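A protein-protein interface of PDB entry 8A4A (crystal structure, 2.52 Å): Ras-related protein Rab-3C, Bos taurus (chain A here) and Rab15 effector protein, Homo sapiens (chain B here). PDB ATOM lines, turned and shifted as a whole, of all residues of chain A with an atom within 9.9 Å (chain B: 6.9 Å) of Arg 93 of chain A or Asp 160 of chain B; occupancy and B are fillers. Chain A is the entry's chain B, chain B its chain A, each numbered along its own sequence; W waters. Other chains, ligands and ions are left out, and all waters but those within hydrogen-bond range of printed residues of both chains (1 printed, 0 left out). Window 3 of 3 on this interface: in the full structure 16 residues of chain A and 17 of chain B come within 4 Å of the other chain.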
ATOM      1  N   SER A  41      27.826  14.171  12.830  1.00  0.00           N
ATOM      2  CA  SER A  41      28.360  15.426  12.324  1.00  0.00           C
ATOM      3  C   SER A  41      28.334  16.487  13.416  1.00  0.00           C
ATOM      4  O   SER A  41      27.425  16.520  14.253  1.00  0.00           O
ATOM      5  CB  SER A  41      27.550  15.892  11.113  1.00  0.00           C
ATOM      6  OG  SER A  41      28.107  17.065  10.551  1.00  0.00           O
ATOM      7  N   SER A  63      32.649  20.954   7.038  1.00  0.00           N
ATOM      8  CA  SER A  63      32.262  19.559   7.149  1.00  0.00           C
ATOM      9  C   SER A  63      33.146  18.681   6.270  1.00  0.00           C
ATOM     10  O   SER A  63      33.522  19.061   5.157  1.00  0.00           O
ATOM     11  CB  SER A  63      30.795  19.392   6.770  1.00  0.00           C
ATOM     12  OG  SER A  63      30.220  18.318   7.487  1.00  0.00           O
ATOM     13  N   THR A  64      33.486  17.504   6.788  1.00  0.00           N
ATOM     14  CA  THR A  64      34.364  16.578   6.089  1.00  0.00           C
ATOM     15  C   THR A  64      33.597  15.814   5.017  1.00  0.00           C
ATOM     16  O   THR A  64      32.509  15.291   5.272  1.00  0.00           O
ATOM     17  CB  THR A  64      34.999  15.604   7.080  1.00  0.00           C
ATOM     18  OG1 THR A  64      35.775  16.338   8.041  1.00  0.00           O
ATOM     19  CG2 THR A  64      35.882  14.586   6.359  1.00  0.00           C
ATOM     20  N   VAL A  65      34.172  15.744   3.821  1.00  0.00           N
ATOM     21  CA  VAL A  65      33.583  15.016   2.706  1.00  0.00           C
ATOM     22  C   VAL A  65      34.245  13.649   2.658  1.00  0.00           C
ATOM     23  O   VAL A  65      35.442  13.536   2.374  1.00  0.00           O
ATOM     24  CB  VAL A  65      33.756  15.765   1.380  1.00  0.00           C
ATOM     25  CG1 VAL A  65      33.117  14.975   0.246  1.00  0.00           C
ATOM     26  CG2 VAL A  65      33.146  17.156   1.479  1.00  0.00           C
ATOM     27  N   GLY A  66      33.479  12.606   2.965  1.00  0.00           N
ATOM     28  CA  GLY A  66      34.013  11.268   2.848  1.00  0.00           C
ATOM     29  C   GLY A  66      34.827  10.888   4.063  1.00  0.00           C
ATOM     30  O   GLY A  66      34.289  10.516   5.108  1.00  0.00           O
ATOM     31  N   ILE A  67      36.146  10.979   3.925  1.00  0.00           N
ATOM     32  CA  ILE A  67      37.065  10.555   4.970  1.00  0.00           C
ATOM     33  C   ILE A  67      38.410  11.193   4.668  1.00  0.00           C
ATOM     34  O   ILE A  67      38.661  11.646   3.551  1.00  0.00           O
ATOM     35  CB  ILE A  67      37.146   9.006   5.031  1.00  0.00           C
ATOM     36  CG1 ILE A  67      37.542   8.532   6.431  1.00  0.00           C
ATOM     37  CG2 ILE A  67      38.098   8.468   3.966  1.00  0.00           C
ATOM     38  CD1 ILE A  67      37.695   7.037   6.542  1.00  0.00           C
ATOM     39  N   ALA A  89      33.497  11.103   8.020  1.00  0.00           N
ATOM     40  CA  ALA A  89      32.391  12.040   7.890  1.00  0.00           C
ATOM     41  C   ALA A  89      31.186  11.528   8.672  1.00  0.00           C
ATOM     42  O   ALA A  89      30.839  10.346   8.596  1.00  0.00           O
ATOM     43  CB  ALA A  89      32.034  12.245   6.420  1.00  0.00           C
ATOM     44  N   GLY A  90      30.554  12.419   9.440  1.00  0.00           N
ATOM     45  CA  GLY A  90      29.405  12.020  10.236  1.00  0.00           C
ATOM     46  C   GLY A  90      28.088  12.000   9.489  1.00  0.00           C
ATOM     47  O   GLY A  90      27.168  11.289   9.903  1.00  0.00           O
ATOM     48  N   GLN A  91      27.978  12.751   8.397  1.00  0.00           N
ATOM     49  CA  GLN A  91      26.727  12.806   7.654  1.00  0.00           C
ATOM     50  C   GLN A  91      26.359  11.431   7.108  1.00  0.00           C
ATOM     51  O   GLN A  91      27.221  10.667   6.664  1.00  0.00           O
ATOM     52  CB  GLN A  91      26.840  13.810   6.511  1.00  0.00           C
ATOM     53  CG  GLN A  91      26.294  15.182   6.846  1.00  0.00           C
ATOM     54  CD  GLN A  91      27.121  16.291   6.229  1.00  0.00           C
ATOM     55  OE1 GLN A  91      27.371  16.305   5.019  1.00  0.00           O
ATOM     56  NE2 GLN A  91      27.552  17.234   7.060  1.00  0.00           N
ATOM     57  N   GLU A  92      25.058  11.125   7.136  1.00  0.00           N
ATOM     58  CA  GLU A  92      24.597   9.797   6.741  1.00  0.00           C
ATOM     59  C   GLU A  92      24.919   9.494   5.281  1.00  0.00           C
ATOM     60  O   GLU A  92      25.138   8.330   4.926  1.00  0.00           O
ATOM     61  CB  GLU A  92      23.092   9.667   6.997  1.00  0.00           C
ATOM     62  CG  GLU A  92      22.661   8.270   7.435  1.00  0.00           C
ATOM     63  CD  GLU A  92      21.193   7.983   7.157  1.00  0.00           C
ATOM     64  OE1 GLU A  92      20.606   8.644   6.274  1.00  0.00           O
ATOM     65  OE2 GLU A  92      20.626   7.088   7.822  1.00  0.00           O
ATOM     66  N   ARG A  93      24.974  10.526   4.433  1.00  0.00           N
ATOM     67  CA  ARG A  93      25.310  10.340   3.023  1.00  0.00           C
ATOM     68  C   ARG A  93      26.650   9.632   2.842  1.00  0.00           C
ATOM     69  O   ARG A  93      26.850   8.922   1.849  1.00  0.00           O
ATOM     70  CB  ARG A  93      25.323  11.699   2.322  1.00  0.00           C
ATOM     71  CG  ARG A  93      26.314  11.834   1.182  1.00  0.00           C
ATOM     72  CD  ARG A  93      26.185  13.191   0.528  1.00  0.00           C
ATOM     73  NE  ARG A  93      24.959  13.293  -0.253  1.00  0.00           N
ATOM     74  CZ  ARG A  93      24.844  12.910  -1.517  1.00  0.00           C
ATOM     75  NH1 ARG A  93      25.881  12.441  -2.193  1.00  0.00           N
ATOM     76  NH2 ARG A  93      23.659  13.003  -2.117  1.00  0.00           N
ATOM     77  N   TYR A  94      27.573   9.799   3.786  1.00  0.00           N
ATOM     78  CA  TYR A  94      28.890   9.186   3.698  1.00  0.00           C
ATOM     79  C   TYR A  94      29.014   7.934   4.561  1.00  0.00           C
ATOM     80  O   TYR A  94      30.133   7.490   4.839  1.00  0.00           O
ATOM     81  CB  TYR A  94      29.965  10.209   4.068  1.00  0.00           C
ATOM     82  CG  TYR A  94      29.886  11.457   3.216  1.00  0.00           C
ATOM     83  CD1 TYR A  94      30.117  11.402   1.846  1.00  0.00           C
ATOM     84  CD2 TYR A  94      29.547  12.681   3.776  1.00  0.00           C
ATOM     85  CE1 TYR A  94      30.031  12.536   1.062  1.00  0.00           C
ATOM     86  CE2 TYR A  94      29.458  13.818   3.002  1.00  0.00           C
ATOM     87  CZ  TYR A  94      29.699  13.742   1.646  1.00  0.00           C
ATOM     88  OH  TYR A  94      29.609  14.880   0.877  1.00  0.00           O
ATOM     89  N   ARG A  95      27.891   7.351   4.986  1.00  0.00           N
ATOM     90  CA  ARG A  95      27.964   6.146   5.807  1.00  0.00           C
ATOM     91  C   ARG A  95      28.687   5.026   5.064  1.00  0.00           C
ATOM     92  O   ARG A  95      29.709   4.510   5.537  1.00  0.00           O
ATOM     93  CB  ARG A  95      26.552   5.715   6.219  1.00  0.00           C
ATOM     94  CG  ARG A  95      26.399   5.220   7.662  1.00  0.00           C
ATOM     95  CD  ARG A  95      27.223   6.027   8.674  1.00  0.00           C
ATOM     96  NE  ARG A  95      26.690   7.362   8.932  1.00  0.00           N
ATOM     97  CZ  ARG A  95      25.796   7.656   9.869  1.00  0.00           C
ATOM     98  NH1 ARG A  95      25.252   6.718  10.629  1.00  0.00           N
ATOM     99  NH2 ARG A  95      25.437   8.926  10.046  1.00  0.00           N
ATOM    100  N   THR A  96      28.226   4.709   3.850  1.00  0.00           N
ATOM    101  CA  THR A  96      28.767   3.571   3.106  1.00  0.00           C
ATOM    102  C   THR A  96      30.269   3.710   2.884  1.00  0.00           C
ATOM    103  O   THR A  96      31.029   2.745   3.051  1.00  0.00           O
ATOM    104  CB  THR A  96      28.049   3.421   1.764  1.00  0.00           C
ATOM    105  OG1 THR A  96      26.640   3.283   1.983  1.00  0.00           O
ATOM    106  CG2 THR A  96      28.555   2.190   1.030  1.00  0.00           C
ATOM    107  N   ILE A  97      30.722   4.901   2.493  1.00  0.00           N
ATOM    108  CA  ILE A  97      32.151   5.070   2.270  1.00  0.00           C
ATOM    109  C   ILE A  97      32.914   4.950   3.586  1.00  0.00           C
ATOM    110  O   ILE A  97      33.943   4.261   3.656  1.00  0.00           O
ATOM    111  CB  ILE A  97      32.441   6.391   1.531  1.00  0.00           C
ATOM    112  CG1 ILE A  97      33.943   6.551   1.303  1.00  0.00           C
ATOM    113  CG2 ILE A  97      31.859   7.594   2.264  1.00  0.00           C
ATOM    114  CD1 ILE A  97      34.281   7.172  -0.025  1.00  0.00           C
ATOM    115  N   THR A  98      32.407   5.561   4.663  1.00  0.00           N
ATOM    116  CA  THR A  98      33.182   5.539   5.901  1.00  0.00           C
ATOM    117  C   THR A  98      33.295   4.119   6.436  1.00  0.00           C
ATOM    118  O   THR A  98      34.384   3.671   6.815  1.00  0.00           O
ATOM    119  CB  THR A  98      32.575   6.471   6.956  1.00  0.00           C
ATOM    120  OG1 THR A  98      31.204   6.126   7.183  1.00  0.00           O
ATOM    121  CG2 THR A  98      32.680   7.926   6.510  1.00  0.00           C
ATOM    122  N   THR A  99      32.184   3.380   6.432  1.00  0.00           N
ATOM    123  CA  THR A  99      32.218   1.999   6.894  1.00  0.00           C
ATOM    124  C   THR A  99      33.106   1.138   6.010  1.00  0.00           C
ATOM    125  O   THR A  99      33.646   0.127   6.476  1.00  0.00           O
ATOM    126  CB  THR A  99      30.800   1.432   6.958  1.00  0.00           C
ATOM    127  OG1 THR A  99      30.175   1.557   5.678  1.00  0.00           O
ATOM    128  CG2 THR A  99      29.979   2.196   7.975  1.00  0.00           C
ATOM    129  N   TRP A 126      26.248   3.784  16.591  1.00  0.00           N
ATOM    130  CA  TRP A 126      27.657   3.800  16.193  1.00  0.00           C
ATOM    131  C   TRP A 126      28.379   2.560  16.710  1.00  0.00           C
ATOM    132  O   TRP A 126      29.211   1.972  16.003  1.00  0.00           O
ATOM    133  CB  TRP A 126      28.343   5.075  16.689  1.00  0.00           C
ATOM    134  CG  TRP A 126      27.916   6.297  15.948  1.00  0.00           C
ATOM    135  CD1 TRP A 126      27.206   7.352  16.447  1.00  0.00           C
ATOM    136  CD2 TRP A 126      28.171   6.601  14.572  1.00  0.00           C
ATOM    137  NE1 TRP A 126      26.997   8.288  15.466  1.00  0.00           N
ATOM    138  CE2 TRP A 126      27.584   7.855  14.306  1.00  0.00           C
ATOM    139  CE3 TRP A 126      28.846   5.938  13.537  1.00  0.00           C
ATOM    140  CZ2 TRP A 126      27.643   8.457  13.051  1.00  0.00           C
ATOM    141  CZ3 TRP A 126      28.905   6.537  12.291  1.00  0.00           C
ATOM    142  CH2 TRP A 126      28.307   7.784  12.058  1.00  0.00           C
ATOM    143  N   THR B  98      29.192  20.123  -5.005  1.00  0.00           N
ATOM    144  CA  THR B  98      27.955  19.708  -4.361  1.00  0.00           C
ATOM    145  C   THR B  98      26.863  20.733  -4.627  1.00  0.00           C
ATOM    146  O   THR B  98      27.034  21.923  -4.331  1.00  0.00           O
ATOM    147  CB  THR B  98      28.149  19.518  -2.856  1.00  0.00           C
ATOM    148  OG1 THR B  98      29.358  18.787  -2.616  1.00  0.00           O
ATOM    149  CG2 THR B  98      26.971  18.774  -2.258  1.00  0.00           C
ATOM    150  N   GLN B 105      19.029  20.067   0.986  1.00  0.00           N
ATOM    151  CA  GLN B 105      19.498  18.704   0.801  1.00  0.00           C
ATOM    152  C   GLN B 105      20.353  18.625  -0.459  1.00  0.00           C
ATOM    153  O   GLN B 105      20.252  19.464  -1.360  1.00  0.00           O
ATOM    154  CB  GLN B 105      18.324  17.723   0.706  1.00  0.00           C
ATOM    155  CG  GLN B 105      17.440  17.677   1.943  1.00  0.00           C
ATOM    156  CD  GLN B 105      18.102  16.964   3.102  1.00  0.00           C
ATOM    157  OE1 GLN B 105      18.584  15.839   2.960  1.00  0.00           O
ATOM    158  NE2 GLN B 105      18.126  17.612   4.260  1.00  0.00           N
ATOM    159  N   ILE B 106      21.202  17.607  -0.518  1.00  0.00           N
ATOM    160  CA  ILE B 106      22.113  17.456  -1.649  1.00  0.00           C
ATOM    161  C   ILE B 106      21.358  16.825  -2.812  1.00  0.00           C
ATOM    162  O   ILE B 106      20.785  15.739  -2.678  1.00  0.00           O
ATOM    163  CB  ILE B 106      23.343  16.624  -1.263  1.00  0.00           C
ATOM    164  CG1 ILE B 106      24.218  17.409  -0.286  1.00  0.00           C
ATOM    165  CG2 ILE B 106      24.135  16.241  -2.498  1.00  0.00           C
ATOM    166  CD1 ILE B 106      25.370  16.619   0.276  1.00  0.00           C
ATOM    167  N   LYS B 107      21.353  17.509  -3.956  1.00  0.00           N
ATOM    168  CA  LYS B 107      20.717  16.984  -5.158  1.00  0.00           C
ATOM    169  C   LYS B 107      21.692  16.255  -6.068  1.00  0.00           C
ATOM    170  O   LYS B 107      21.298  15.293  -6.739  1.00  0.00           O
ATOM    171  CB  LYS B 107      20.053  18.114  -5.952  1.00  0.00           C
ATOM    172  CG  LYS B 107      19.026  18.925  -5.177  1.00  0.00           C
ATOM    173  CD  LYS B 107      17.908  18.048  -4.619  1.00  0.00           C
ATOM    174  CE  LYS B 107      17.127  18.779  -3.529  1.00  0.00           C
ATOM    175  NZ  LYS B 107      16.214  17.879  -2.767  1.00  0.00           N
ATOM    176  N   LEU B 108      22.952  16.684  -6.107  1.00  0.00           N
ATOM    177  CA  LEU B 108      23.903  16.166  -7.078  1.00  0.00           C
ATOM    178  C   LEU B 108      25.320  16.455  -6.607  1.00  0.00           C
ATOM    179  O   LEU B 108      25.595  17.522  -6.055  1.00  0.00           O
ATOM    180  CB  LEU B 108      23.667  16.790  -8.459  1.00  0.00           C
ATOM    181  CG  LEU B 108      24.616  16.385  -9.584  1.00  0.00           C
ATOM    182  CD1 LEU B 108      24.340  14.959 -10.025  1.00  0.00           C
ATOM    183  CD2 LEU B 108      24.492  17.353 -10.751  1.00  0.00           C
ATOM    184  N   GLN B 109      26.215  15.498  -6.823  1.00  0.00           N
ATOM    185  CA  GLN B 109      27.635  15.715  -6.589  1.00  0.00           C
ATOM    186  C   GLN B 109      28.393  15.318  -7.841  1.00  0.00           C
ATOM    187  O   GLN B 109      28.128  14.261  -8.418  1.00  0.00           O
ATOM    188  CB  GLN B 109      28.146  14.924  -5.381  1.00  0.00           C
ATOM    189  CG  GLN B 109      27.924  15.630  -4.060  1.00  0.00           C
ATOM    190  CD  GLN B 109      28.487  14.859  -2.885  1.00  0.00           C
ATOM    191  OE1 GLN B 109      28.364  13.638  -2.808  1.00  0.00           O
ATOM    192  NE2 GLN B 109      29.120  15.575  -1.962  1.00  0.00           N
ATOM    193  N   LEU B 110      29.310  16.177  -8.270  1.00  0.00           N
ATOM    194  CA  LEU B 110      30.194  15.898  -9.395  1.00  0.00           C
ATOM    195  C   LEU B 110      31.597  15.717  -8.842  1.00  0.00           C
ATOM    196  O   LEU B 110      32.192  16.674  -8.335  1.00  0.00           O
ATOM    197  CB  LEU B 110      30.152  17.022 -10.426  1.00  0.00           C
ATOM    198  CG  LEU B 110      28.849  17.208 -11.198  1.00  0.00           C
ATOM    199  CD1 LEU B 110      29.038  18.196 -12.333  1.00  0.00           C
ATOM    200  CD2 LEU B 110      28.357  15.877 -11.726  1.00  0.00           C
ATOM    201  N   CYS B 154      32.562   6.931  -6.580  1.00  0.00           N
ATOM    202  CA  CYS B 154      31.203   7.247  -7.008  1.00  0.00           C
ATOM    203  C   CYS B 154      30.234   6.132  -6.640  1.00  0.00           C
ATOM    204  O   CYS B 154      29.074   6.395  -6.297  1.00  0.00           O
ATOM    205  CB  CYS B 154      31.173   7.514  -8.511  1.00  0.00           C
ATOM    206  SG  CYS B 154      31.892   9.104  -8.972  1.00  0.00           S
ATOM    207  N   LEU B 156      30.494   4.228  -3.967  1.00  0.00           N
ATOM    208  CA  LEU B 156      30.283   4.295  -2.526  1.00  0.00           C
ATOM    209  C   LEU B 156      29.399   5.470  -2.134  1.00  0.00           C
ATOM    210  O   LEU B 156      28.638   5.374  -1.164  1.00  0.00           O
ATOM    211  CB  LEU B 156      31.626   4.384  -1.810  1.00  0.00           C
ATOM    212  CG  LEU B 156      32.488   3.124  -1.812  1.00  0.00           C
ATOM    213  CD1 LEU B 156      33.916   3.493  -1.477  1.00  0.00           C
ATOM    214  CD2 LEU B 156      31.948   2.099  -0.820  1.00  0.00           C
ATOM    215  N   ILE B 157      29.502   6.595  -2.846  1.00  0.00           N
ATOM    216  CA  ILE B 157      28.680   7.751  -2.505  1.00  0.00           C
ATOM    217  C   ILE B 157      27.220   7.507  -2.875  1.00  0.00           C
ATOM    218  O   ILE B 157      26.312   7.824  -2.097  1.00  0.00           O
ATOM    219  CB  ILE B 157      29.231   9.025  -3.166  1.00  0.00           C
ATOM    220  CG1 ILE B 157      30.662   9.291  -2.693  1.00  0.00           C
ATOM    221  CG2 ILE B 157      28.344  10.213  -2.830  1.00  0.00           C
ATOM    222  CD1 ILE B 157      30.810   9.343  -1.185  1.00  0.00           C
ATOM    223  N   GLY B 158      26.963   6.950  -4.066  1.00  0.00           N
ATOM    224  CA  GLY B 158      25.618   6.542  -4.410  1.00  0.00           C
ATOM    225  C   GLY B 158      25.199   7.030  -5.784  1.00  0.00           C
ATOM    226  O   GLY B 158      26.031   7.410  -6.617  1.00  0.00           O
ATOM    227  N   GLU B 159      23.879   7.024  -6.005  1.00  0.00           N
ATOM    228  CA  GLU B 159      23.330   7.209  -7.347  1.00  0.00           C
ATOM    229  C   GLU B 159      23.416   8.656  -7.821  1.00  0.00           C
ATOM    230  O   GLU B 159      23.475   8.900  -9.032  1.00  0.00           O
ATOM    231  CB  GLU B 159      21.879   6.725  -7.385  1.00  0.00           C
ATOM    232  CG  GLU B 159      21.140   6.895  -6.059  1.00  0.00           C
ATOM    233  CD  GLU B 159      19.646   6.639  -6.173  1.00  0.00           C
ATOM    234  OE1 GLU B 159      19.258   5.476  -6.415  1.00  0.00           O
ATOM    235  OE2 GLU B 159      18.859   7.597  -6.008  1.00  0.00           O
ATOM    236  N   ASP B 160      23.413   9.626  -6.904  1.00  0.00           N
ATOM    237  CA  ASP B 160      23.427  11.034  -7.278  1.00  0.00           C
ATOM    238  C   ASP B 160      24.833  11.628  -7.272  1.00  0.00           C
ATOM    239  O   ASP B 160      24.989  12.852  -7.192  1.00  0.00           O
ATOM    240  CB  ASP B 160      22.497  11.841  -6.369  1.00  0.00           C
ATOM    241  CG  ASP B 160      22.800  11.652  -4.895  1.00  0.00           C
ATOM    242  OD1 ASP B 160      23.785  10.959  -4.557  1.00  0.00           O
ATOM    243  OD2 ASP B 160      22.031  12.191  -4.068  1.00  0.00           O
ATOM    244  N   CYS B 161      25.856  10.783  -7.354  1.00  0.00           N
ATOM    245  CA  CYS B 161      27.240  11.209  -7.499  1.00  0.00           C
ATOM    246  C   CYS B 161      27.749  10.754  -8.860  1.00  0.00           C
ATOM    247  O   CYS B 161      27.663   9.567  -9.193  1.00  0.00           O
ATOM    248  CB  CYS B 161      28.108  10.634  -6.381  1.00  0.00           C
ATOM    249  SG  CYS B 161      29.871  10.992  -6.534  1.00  0.00           S
ATOM    250  N   LEU B 162      28.273  11.695  -9.641  1.00  0.00           N
ATOM    251  CA  LEU B 162      28.709  11.447 -11.008  1.00  0.00           C
ATOM    252  C   LEU B 162      30.204  11.686 -11.121  1.00  0.00           C
ATOM    253  O   LEU B 162      30.701  12.735 -10.700  1.00  0.00           O
ATOM    254  CB  LEU B 162      27.984  12.361 -11.994  1.00  0.00           C
ATOM    255  CG  LEU B 162      26.767  11.817 -12.732  1.00  0.00           C
ATOM    256  CD1 LEU B 162      25.668  11.444 -11.744  1.00  0.00           C
ATOM    257  CD2 LEU B 162      26.276  12.841 -13.741  1.00  0.00           C
ATOM    258  N   LYS B 224      17.591  13.409 -11.701  1.00  0.00           N
ATOM    259  CA  LYS B 224      18.901  12.792 -11.880  1.00  0.00           C
ATOM    260  C   LYS B 224      18.844  11.786 -13.020  1.00  0.00           C
ATOM    261  O   LYS B 224      18.627  10.587 -12.812  1.00  0.00           O
ATOM    262  CB  LYS B 224      19.383  12.141 -10.581  1.00  0.00           C
ATOM    263  CG  LYS B 224      20.045  13.120  -9.616  1.00  0.00           C
ATOM    264  CD  LYS B 224      19.038  13.746  -8.657  1.00  0.00           C
ATOM    265  CE  LYS B 224      18.851  12.890  -7.416  1.00  0.00           C
ATOM    266  NZ  LYS B 224      18.007  13.574  -6.397  1.00  0.00           N
ATOM    267  N   LEU B 227      23.022  10.369 -15.601  1.00  0.00           N
ATOM    268  CA  LEU B 227      23.894   9.253 -15.243  1.00  0.00           C
ATOM    269  C   LEU B 227      24.020   8.259 -16.395  1.00  0.00           C
ATOM    270  O   LEU B 227      25.088   8.151 -17.006  1.00  0.00           O
ATOM    271  CB  LEU B 227      23.365   8.569 -13.973  1.00  0.00           C
ATOM    272  CG  LEU B 227      24.143   7.501 -13.189  1.00  0.00           C
ATOM    273  CD1 LEU B 227      24.140   6.145 -13.896  1.00  0.00           C
ATOM    274  CD2 LEU B 227      25.570   7.953 -12.903  1.00  0.00           C
HETATM  275  O   HOH W   1      28.803   6.794   1.406  1.00  0.00           O
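The guanidinium group (NH1) of Arg 93 of chain A sits at hydrogen-bond distance from the side-chain amide oxygen (OE1) of Gln 109 of chain B, 2.8 Å away.
NE2 of Gln 109 of chain B is in hydrogen-bond range of OH of Tyr 94 of chain A.
NH2 of Arg 93 of chain A lies within salt-bridge range of OD2 of Asp 160 of chain B (2.7 Å).
NE2 of Gln 109 of chain B sits at hydrogen-bond distance from OG1 of Thr 98 of chain B, 3.3 Å away.
The backbone NH (N) of Gln 109 of chain B lies within hydrogen-bond range of the backbone carbonyl oxygen (O) of Asp 160 of chain B (2.9 Å).
O of Gln 109 of chain B lies within hydrogen-bond range of N of Leu 162 of chain B.
O of Tyr 94 of chain A sits at hydrogen-bond distance from OG1 of Thr 98 of chain A (2.9 Å).
O of Thr 96 of chain A sits at hydrogen-bond distance from OG1 of Thr 99 of chain A (3.0 Å).
Ile 106 of chain B touches Arg 93 of chain A (CG2 to NH2, 3.3 Å).
Ile 157 of chain B touches Arg 93 of chain A.
CD1 of Tyr 94 of chain A touches CD1 of Ile 157 of chain B, at 3.7 Å.
O of Leu 156 of chain B touches CB of Thr 96 of chain A (3.6 Å).
Ile 97 of chain A touches Leu 156 of chain B.
Val 65 of chain A touches none of the printed residues of chain B.
Arg 93 of chain A touches just these residues of chain B: Ile 106 (3.3 Å), Gln 109 (2.8 Å), Ile 157 (3.4 Å) and Asp 160 (2.7 Å).
Of the printed residues of chain B, Tyr 94 of chain A touches Gln 109 (3.0 Å) and Ile 157 (3.7 Å).
Of the printed residues of chain B, Thr 96 of chain A touches Leu 156.
Of the printed residues of chain B, Ile 97 of chain A touches Leu 156.
Ile 106 of chain B touches just one residue of chain A: Arg 93 (3.3 Å).
Of chain A, only Arg 93 (2.8 Å) and Tyr 94 (3.0 Å) come within 4 Å of Gln 109 of chain B.
Printed residues of chain A within 4 Å of Leu 156 of chain B: Thr 96 and Ile 97.
Of the printed residues of chain A, Ile 157 of chain B touches Arg 93 (3.4 Å) and Tyr 94 (3.7 Å).
Asp 160 of chain B touches one residue of chain A.
No residue of chain A comes within 4 Å of Cys 161 of chain B.
The nearest residue of chain B that does not touch Arg 93 of chain A is Leu 156 of chain B (5.0 Å).
The nearest residue of chain A that does not touch Asp 160 of chain B is Tyr 94 of chain A (8.5 Å).
Of the 18 printed residues of chain A, 4 touch a printed residue of chain B.
Hydrophobic or aromatic side chains of chain A within 4 Å of the printed part of chain B: Tyr 94 and Ile 97.
Of the 17 printed residues of chain B, 5 touch a printed residue of chain A.
Hydrophobic or aromatic side chains of chain B within 4 Å of the printed part of chain A: Ile 106, Leu 156 and Ile 157.
Among the printed residues, 8 pairs touch across the chains.
Water W1 lies within hydrogen-bond range of the backbone NH of Ile 97 of chain A (2.9 Å), the backbone carbonyl oxygen of Arg 93 of chain A (2.9 Å), the backbone carbonyl oxygen of Leu 156 of chain B (2.9 Å) and the backbone NH of Thr 96 of chain A (3.3 Å).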
